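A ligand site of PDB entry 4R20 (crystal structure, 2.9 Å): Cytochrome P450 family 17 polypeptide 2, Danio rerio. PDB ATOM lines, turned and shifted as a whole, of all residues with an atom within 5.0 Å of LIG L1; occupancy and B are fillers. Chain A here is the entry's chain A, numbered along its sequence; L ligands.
OD1 of Asn 194 lies within hydrogen-bond range of O1 of LIG L1 (3.4 Å). The side-chain sulfur (SG) of Cys 425 is bound to an iron atom (FE1) of LG2 L2 (2.3 Å).
N1 of LIG L1 is bound to FE1 of LG2 L2, 1.9 Å away.
The side-chain carboxylate (OE1) of Glu 283 is in hydrogen-bond range of the backbone NH (N) of Ala 105 (3.1 Å).
Residues that only touch LIG L1: Ala 105 (3.7 Å), Ile 197 (3.4 Å), Glu 283 (3.9 Å), Gly 286 (3.8 Å), Thr 291 (3.2 Å), Val 351 (3.8 Å) and Ser 352 (3.6 Å). Hydrophobic or aromatic side chains that line LIG L1: Ala 105, Ile 197 and Val 351. Of the 20 residues printed, 8 come within 4 Å of LIG L1.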
ATOM      1  N   LEU A  97       6.809  12.890   1.518  1.00  0.00           N
ATOM      2  CA  LEU A  97       5.907  13.707   0.720  1.00  0.00           C
ATOM      3  C   LEU A  97       5.276  12.936  -0.438  1.00  0.00           C
ATOM      4  O   LEU A  97       4.066  12.985  -0.631  1.00  0.00           O
ATOM      5  CB  LEU A  97       6.662  14.941   0.201  1.00  0.00           C
ATOM      6  CG  LEU A  97       6.436  16.304   0.894  1.00  0.00           C
ATOM      7  CD1 LEU A  97       5.783  16.230   2.285  1.00  0.00           C
ATOM      8  CD2 LEU A  97       7.742  17.071   0.943  1.00  0.00           C
ATOM      9  N   ALA A 105       7.821  16.069  -9.297  1.00  0.00           N
ATOM     10  CA  ALA A 105       8.892  17.022  -8.976  1.00  0.00           C
ATOM     11  C   ALA A 105      10.111  16.388  -8.334  1.00  0.00           C
ATOM     12  O   ALA A 105      11.209  16.903  -8.486  1.00  0.00           O
ATOM     13  CB  ALA A 105       8.376  18.131  -8.079  1.00  0.00           C
ATOM     14  N   PHE A 106       9.934  15.304  -7.604  1.00  0.00           N
ATOM     15  CA  PHE A 106      11.071  14.675  -6.935  1.00  0.00           C
ATOM     16  C   PHE A 106      11.349  13.257  -7.449  1.00  0.00           C
ATOM     17  O   PHE A 106      12.070  12.475  -6.827  1.00  0.00           O
ATOM     18  CB  PHE A 106      10.864  14.695  -5.409  1.00  0.00           C
ATOM     19  CG  PHE A 106      10.520  16.066  -4.855  1.00  0.00           C
ATOM     20  CD1 PHE A 106      11.482  17.071  -4.817  1.00  0.00           C
ATOM     21  CD2 PHE A 106       9.258  16.337  -4.347  1.00  0.00           C
ATOM     22  CE1 PHE A 106      11.172  18.329  -4.302  1.00  0.00           C
ATOM     23  CE2 PHE A 106       8.952  17.581  -3.828  1.00  0.00           C
ATOM     24  CZ  PHE A 106       9.912  18.583  -3.804  1.00  0.00           C
ATOM     25  N   ASN A 194      -2.018  21.179   5.294  1.00  0.00           N
ATOM     26  CA  ASN A 194      -1.043  21.886   4.456  1.00  0.00           C
ATOM     27  C   ASN A 194      -0.092  22.692   5.312  1.00  0.00           C
ATOM     28  O   ASN A 194       1.131  22.586   5.159  1.00  0.00           O
ATOM     29  CB  ASN A 194      -1.718  22.831   3.449  1.00  0.00           C
ATOM     30  CG  ASN A 194      -2.044  22.154   2.123  1.00  0.00           C
ATOM     31  OD1 ASN A 194      -1.351  21.231   1.661  1.00  0.00           O
ATOM     32  ND2 ASN A 194      -3.099  22.629   1.472  1.00  0.00           N
ATOM     33  N   ILE A 197       2.375  20.393   7.270  1.00  0.00           N
ATOM     34  CA  ILE A 197       3.465  19.930   6.417  1.00  0.00           C
ATOM     35  C   ILE A 197       4.489  21.035   6.137  1.00  0.00           C
ATOM     36  O   ILE A 197       5.694  20.829   6.314  1.00  0.00           O
ATOM     37  CB  ILE A 197       2.916  19.389   5.081  1.00  0.00           C
ATOM     38  CG1 ILE A 197       2.183  18.069   5.342  1.00  0.00           C
ATOM     39  CG2 ILE A 197       4.048  19.166   4.080  1.00  0.00           C
ATOM     40  CD1 ILE A 197       1.299  17.581   4.220  1.00  0.00           C
ATOM     41  N   VAL A 198       3.991  22.208   5.707  1.00  0.00           N
ATOM     42  CA  VAL A 198       4.871  23.347   5.431  1.00  0.00           C
ATOM     43  C   VAL A 198       5.708  23.709   6.649  1.00  0.00           C
ATOM     44  O   VAL A 198       6.917  23.887   6.533  1.00  0.00           O
ATOM     45  CB  VAL A 198       4.080  24.600   4.991  1.00  0.00           C
ATOM     46  CG1 VAL A 198       4.950  25.853   5.103  1.00  0.00           C
ATOM     47  CG2 VAL A 198       3.556  24.447   3.572  1.00  0.00           C
ATOM     48  N   ILE A 201       8.386  21.226   7.713  1.00  0.00           N
ATOM     49  CA  ILE A 201       9.568  21.347   6.858  1.00  0.00           C
ATOM     50  C   ILE A 201      10.305  22.658   7.150  1.00  0.00           C
ATOM     51  O   ILE A 201      11.525  22.703   7.157  1.00  0.00           O
ATOM     52  CB  ILE A 201       9.193  21.294   5.356  1.00  0.00           C
ATOM     53  CG1 ILE A 201       8.618  19.922   4.992  1.00  0.00           C
ATOM     54  CG2 ILE A 201      10.406  21.580   4.491  1.00  0.00           C
ATOM     55  CD1 ILE A 201       7.771  19.949   3.737  1.00  0.00           C
ATOM     56  N   ARG A 231      -3.371  13.622   4.585  1.00  0.00           N
ATOM     57  CA  ARG A 231      -3.552  14.032   3.207  1.00  0.00           C
ATOM     58  C   ARG A 231      -3.756  12.807   2.317  1.00  0.00           C
ATOM     59  O   ARG A 231      -4.621  12.808   1.445  1.00  0.00           O
ATOM     60  CB  ARG A 231      -2.334  14.843   2.761  1.00  0.00           C
ATOM     61  CG  ARG A 231      -2.373  15.365   1.333  1.00  0.00           C
ATOM     62  CD  ARG A 231      -0.963  15.595   0.782  1.00  0.00           C
ATOM     63  NE  ARG A 231      -0.268  14.335   0.520  1.00  0.00           N
ATOM     64  CZ  ARG A 231       0.989  14.221   0.102  1.00  0.00           C
ATOM     65  NH1 ARG A 231       1.744  15.282  -0.099  1.00  0.00           N
ATOM     66  NH2 ARG A 231       1.494  13.003  -0.103  1.00  0.00           N
ATOM     67  N   ALA A 282      -1.934  14.991  -5.214  1.00  0.00           N
ATOM     68  CA  ALA A 282      -1.449  15.567  -3.970  1.00  0.00           C
ATOM     69  C   ALA A 282      -0.454  16.738  -4.192  1.00  0.00           C
ATOM     70  O   ALA A 282      -0.460  17.718  -3.438  1.00  0.00           O
ATOM     71  CB  ALA A 282      -0.828  14.468  -3.094  1.00  0.00           C
ATOM     72  N   GLU A 283       0.368  16.606  -5.227  1.00  0.00           N
ATOM     73  CA  GLU A 283       1.388  17.581  -5.605  1.00  0.00           C
ATOM     74  C   GLU A 283       0.837  18.815  -6.281  1.00  0.00           C
ATOM     75  O   GLU A 283       1.365  19.919  -6.128  1.00  0.00           O
ATOM     76  CB  GLU A 283       2.388  16.950  -6.574  1.00  0.00           C
ATOM     77  CG  GLU A 283       3.573  17.827  -6.926  1.00  0.00           C
ATOM     78  CD  GLU A 283       4.748  17.033  -7.434  1.00  0.00           C
ATOM     79  OE1 GLU A 283       4.873  16.901  -8.666  1.00  0.00           O
ATOM     80  OE2 GLU A 283       5.539  16.519  -6.596  1.00  0.00           O
ATOM     81  N   GLY A 286      -0.205  21.094  -3.498  1.00  0.00           N
ATOM     82  CA  GLY A 286       0.904  21.755  -2.868  1.00  0.00           C
ATOM     83  C   GLY A 286       1.320  22.870  -3.758  1.00  0.00           C
ATOM     84  O   GLY A 286       1.316  24.011  -3.341  1.00  0.00           O
ATOM     85  N   ALA A 287       1.608  22.530  -5.015  1.00  0.00           N
ATOM     86  CA  ALA A 287       2.129  23.454  -6.010  1.00  0.00           C
ATOM     87  C   ALA A 287       1.150  24.536  -6.396  1.00  0.00           C
ATOM     88  O   ALA A 287       1.497  25.700  -6.500  1.00  0.00           O
ATOM     89  CB  ALA A 287       2.526  22.687  -7.258  1.00  0.00           C
ATOM     90  N   GLU A 290       0.474  26.919  -2.961  1.00  0.00           N
ATOM     91  CA  GLU A 290       1.582  27.542  -2.268  1.00  0.00           C
ATOM     92  C   GLU A 290       2.291  28.541  -3.205  1.00  0.00           C
ATOM     93  O   GLU A 290       2.526  29.672  -2.806  1.00  0.00           O
ATOM     94  CB  GLU A 290       2.500  26.441  -1.696  1.00  0.00           C
ATOM     95  CG  GLU A 290       3.233  26.804  -0.410  1.00  0.00           C
ATOM     96  CD  GLU A 290       2.342  26.990   0.808  1.00  0.00           C
ATOM     97  OE1 GLU A 290       1.290  26.301   0.906  1.00  0.00           O
ATOM     98  OE2 GLU A 290       2.714  27.819   1.671  1.00  0.00           O
ATOM     99  N   THR A 291       2.584  28.146  -4.447  1.00  0.00           N
ATOM    100  CA  THR A 291       3.137  29.110  -5.442  1.00  0.00           C
ATOM    101  C   THR A 291       2.262  30.325  -5.747  1.00  0.00           C
ATOM    102  O   THR A 291       2.750  31.442  -5.895  1.00  0.00           O
ATOM    103  CB  THR A 291       3.325  28.472  -6.816  1.00  0.00           C
ATOM    104  OG1 THR A 291       2.163  27.721  -7.124  1.00  0.00           O
ATOM    105  CG2 THR A 291       4.495  27.568  -6.862  1.00  0.00           C
ATOM    106  N   VAL A 351       9.988  32.216  -6.579  1.00  0.00           N
ATOM    107  CA  VAL A 351       9.293  31.371  -5.641  1.00  0.00           C
ATOM    108  C   VAL A 351      10.270  30.360  -5.083  1.00  0.00           C
ATOM    109  O   VAL A 351      10.147  29.982  -3.929  1.00  0.00           O
ATOM    110  CB  VAL A 351       8.059  30.654  -6.230  1.00  0.00           C
ATOM    111  CG1 VAL A 351       6.885  31.606  -6.263  1.00  0.00           C
ATOM    112  CG2 VAL A 351       8.317  30.039  -7.588  1.00  0.00           C
ATOM    113  N   SER A 352      11.251  29.978  -5.904  1.00  0.00           N
ATOM    114  CA  SER A 352      12.375  29.114  -5.509  1.00  0.00           C
ATOM    115  C   SER A 352      13.654  29.758  -6.034  1.00  0.00           C
ATOM    116  O   SER A 352      14.055  29.528  -7.190  1.00  0.00           O
ATOM    117  CB  SER A 352      12.225  27.723  -6.117  1.00  0.00           C
ATOM    118  OG  SER A 352      10.898  27.274  -5.919  1.00  0.00           O
ATOM    119  N   ILE A 356      14.793  23.106  -7.421  1.00  0.00           N
ATOM    120  CA  ILE A 356      14.911  21.764  -6.892  1.00  0.00           C
ATOM    121  C   ILE A 356      16.176  21.213  -7.502  1.00  0.00           C
ATOM    122  O   ILE A 356      16.386  21.339  -8.707  1.00  0.00           O
ATOM    123  CB  ILE A 356      13.685  20.895  -7.273  1.00  0.00           C
ATOM    124  CG1 ILE A 356      12.392  21.533  -6.772  1.00  0.00           C
ATOM    125  CG2 ILE A 356      13.795  19.487  -6.696  1.00  0.00           C
ATOM    126  CD1 ILE A 356      11.137  20.961  -7.391  1.00  0.00           C
ATOM    127  N   CYS A 425       8.527  23.963 -15.273  1.00  0.00           N
ATOM    128  CA  CYS A 425       7.286  23.953 -14.479  1.00  0.00           C
ATOM    129  C   CYS A 425       6.135  23.340 -15.236  1.00  0.00           C
ATOM    130  O   CYS A 425       5.871  23.743 -16.355  1.00  0.00           O
ATOM    131  CB  CYS A 425       6.882  25.369 -14.107  1.00  0.00           C
ATOM    132  SG  CYS A 425       5.457  25.411 -13.003  1.00  0.00           S
ATOM    133  N   VAL A 465       8.394  26.663   2.194  1.00  0.00           N
ATOM    134  CA  VAL A 465       8.964  25.874   1.083  1.00  0.00           C
ATOM    135  C   VAL A 465       9.028  26.632  -0.240  1.00  0.00           C
ATOM    136  O   VAL A 465       9.380  26.081  -1.292  1.00  0.00           O
ATOM    137  CB  VAL A 465       8.099  24.618   0.861  1.00  0.00           C
ATOM    138  CG1 VAL A 465       8.205  23.691   2.060  1.00  0.00           C
ATOM    139  CG2 VAL A 465       6.643  24.992   0.617  1.00  0.00           C
ATOM    140  N   VAL A 466       8.647  27.888  -0.180  1.00  0.00           N
ATOM    141  CA  VAL A 466       8.791  28.801  -1.272  1.00  0.00           C
ATOM    142  C   VAL A 466       9.203  30.147  -0.660  1.00  0.00           C
ATOM    143  O   VAL A 466       9.192  30.316   0.559  1.00  0.00           O
ATOM    144  CB  VAL A 466       7.471  28.880  -2.059  1.00  0.00           C
ATOM    145  CG1 VAL A 466       7.180  27.554  -2.731  1.00  0.00           C
ATOM    146  CG2 VAL A 466       6.312  29.230  -1.155  1.00  0.00           C
HETATM  147  C1  LIG L   1       3.846  22.090  -0.424  1.00  0.00           C
HETATM  148  C2  LIG L   1       3.265  21.483   0.831  1.00  0.00           C
HETATM  149  C3  LIG L   1       2.476  20.266   0.489  1.00  0.00           C
HETATM  150  O1  LIG L   1       1.801  19.914   1.691  1.00  0.00           O
HETATM  151  C4  LIG L   1       3.468  19.222   0.011  1.00  0.00           C
HETATM  152  C5  LIG L   1       4.118  19.767  -1.240  1.00  0.00           C
HETATM  153  C6  LIG L   1       4.119  19.003  -2.344  1.00  0.00           C
HETATM  154  C7  LIG L   1       4.796  19.419  -3.630  1.00  0.00           C
HETATM  155  C8  LIG L   1       5.625  20.679  -3.501  1.00  0.00           C
HETATM  156  C9  LIG L   1       4.877  21.690  -2.639  1.00  0.00           C
HETATM  157  C10 LIG L   1       4.756  21.147  -1.200  1.00  0.00           C
HETATM  158  C11 LIG L   1       5.425  23.140  -2.735  1.00  0.00           C
HETATM  159  C12 LIG L   1       6.006  23.637  -4.100  1.00  0.00           C
HETATM  160  C13 LIG L   1       6.776  22.548  -4.810  1.00  0.00           C
HETATM  161  C14 LIG L   1       5.834  21.336  -4.854  1.00  0.00           C
HETATM  162  C15 LIG L   1       6.301  20.442  -5.993  1.00  0.00           C
HETATM  163  C16 LIG L   1       6.568  21.505  -7.048  1.00  0.00           C
HETATM  164  C17 LIG L   1       7.223  22.675  -6.300  1.00  0.00           C
HETATM  165  C18 LIG L   1       8.055  22.322  -3.988  1.00  0.00           C
HETATM  166  C19 LIG L   1       6.091  20.975  -0.471  1.00  0.00           C
HETATM  167  C20 LIG L   1       7.119  23.977  -7.011  1.00  0.00           C
HETATM  168  C21 LIG L   1       6.580  24.098  -8.281  1.00  0.00           C
HETATM  169  N1  LIG L   1       6.547  25.253  -8.967  1.00  0.00           N
HETATM  170  C22 LIG L   1       7.081  26.337  -8.398  1.00  0.00           C
HETATM  171  C23 LIG L   1       7.682  26.289  -7.153  1.00  0.00           C
HETATM  172  C24 LIG L   1       7.704  25.094  -6.463  1.00  0.00           C
HETATM  173  C1  LG2 L   2       8.702  23.202 -11.261  1.00  0.00           C
HETATM  174  C2  LG2 L   2       8.344  27.980 -11.382  1.00  0.00           C
HETATM  175  C3  LG2 L   2       3.641  27.543 -10.275  1.00  0.00           C
HETATM  176  C4  LG2 L   2       3.982  22.766 -10.600  1.00  0.00           C
HETATM  177  C5  LG2 L   2       9.002  24.507 -11.377  1.00  0.00           C
HETATM  178  C6  LG2 L   2      10.292  25.035 -11.615  1.00  0.00           C
HETATM  179  C7  LG2 L   2      10.173  26.365 -11.627  1.00  0.00           C
HETATM  180  C8  LG2 L   2       8.826  26.692 -11.442  1.00  0.00           C
HETATM  181  C9  LG2 L   2      11.275  27.341 -11.814  1.00  0.00           C
HETATM  182  C10 LG2 L   2      11.566  24.237 -11.691  1.00  0.00           C
HETATM  183  C11 LG2 L   2      12.376  24.208 -12.973  1.00  0.00           C
HETATM  184  C12 LG2 L   2      13.403  23.097 -12.797  1.00  0.00           C
HETATM  185  O1  LG2 L   2      14.114  22.781 -13.773  1.00  0.00           O
HETATM  186  O2  LG2 L   2      13.552  22.475 -11.697  1.00  0.00           O
HETATM  187  C13 LG2 L   2       7.019  28.250 -11.082  1.00  0.00           C
HETATM  188  C14 LG2 L   2       6.527  29.572 -10.964  1.00  0.00           C
HETATM  189  C15 LG2 L   2       5.204  29.505 -10.654  1.00  0.00           C
HETATM  190  C16 LG2 L   2       4.886  28.054 -10.557  1.00  0.00           C
HETATM  191  C17 LG2 L   2       7.268  30.859 -11.150  1.00  0.00           C
HETATM  192  C18 LG2 L   2       4.372  30.696 -10.450  1.00  0.00           C
HETATM  193  C19 LG2 L   2       3.106  30.679 -10.034  1.00  0.00           C
HETATM  194  C20 LG2 L   2       3.316  26.200 -10.316  1.00  0.00           C
HETATM  195  C21 LG2 L   2       2.019  25.722 -10.179  1.00  0.00           C
HETATM  196  C22 LG2 L   2       2.074  24.347 -10.244  1.00  0.00           C
HETATM  197  C23 LG2 L   2       3.438  24.005 -10.478  1.00  0.00           C
HETATM  198  C24 LG2 L   2       0.780  26.548  -9.966  1.00  0.00           C
HETATM  199  C25 LG2 L   2       0.873  23.513 -10.197  1.00  0.00           C
HETATM  200  C26 LG2 L   2       0.815  22.236 -10.565  1.00  0.00           C
HETATM  201  C27 LG2 L   2       5.329  22.559 -10.788  1.00  0.00           C
HETATM  202  C28 LG2 L   2       5.864  21.203 -10.820  1.00  0.00           C
HETATM  203  C29 LG2 L   2       7.190  21.328 -11.013  1.00  0.00           C
HETATM  204  C30 LG2 L   2       7.431  22.772 -11.080  1.00  0.00           C
HETATM  205  C31 LG2 L   2       5.101  19.913 -10.711  1.00  0.00           C
HETATM  206  C32 LG2 L   2       8.229  20.244 -11.183  1.00  0.00           C
HETATM  207  C33 LG2 L   2       8.603  20.205 -12.674  1.00  0.00           C
HETATM  208  C34 LG2 L   2       9.527  19.059 -13.023  1.00  0.00           C
HETATM  209  O3  LG2 L   2       9.651  18.702 -14.216  1.00  0.00           O
HETATM  210  O4  LG2 L   2      10.155  18.445 -12.122  1.00  0.00           O
HETATM  211  N1  LG2 L   2       8.113  25.507 -11.242  1.00  0.00           N
HETATM  212  N2  LG2 L   2       6.023  27.386 -10.838  1.00  0.00           N
HETATM  213  N3  LG2 L   2       4.160  25.151 -10.478  1.00  0.00           N
HETATM  214  N4  LG2 L   2       6.299  23.463 -10.929  1.00  0.00           N
HETATM  215 FE1  LG2 L   2       6.177  25.307 -10.872  1.00  0.00          FE
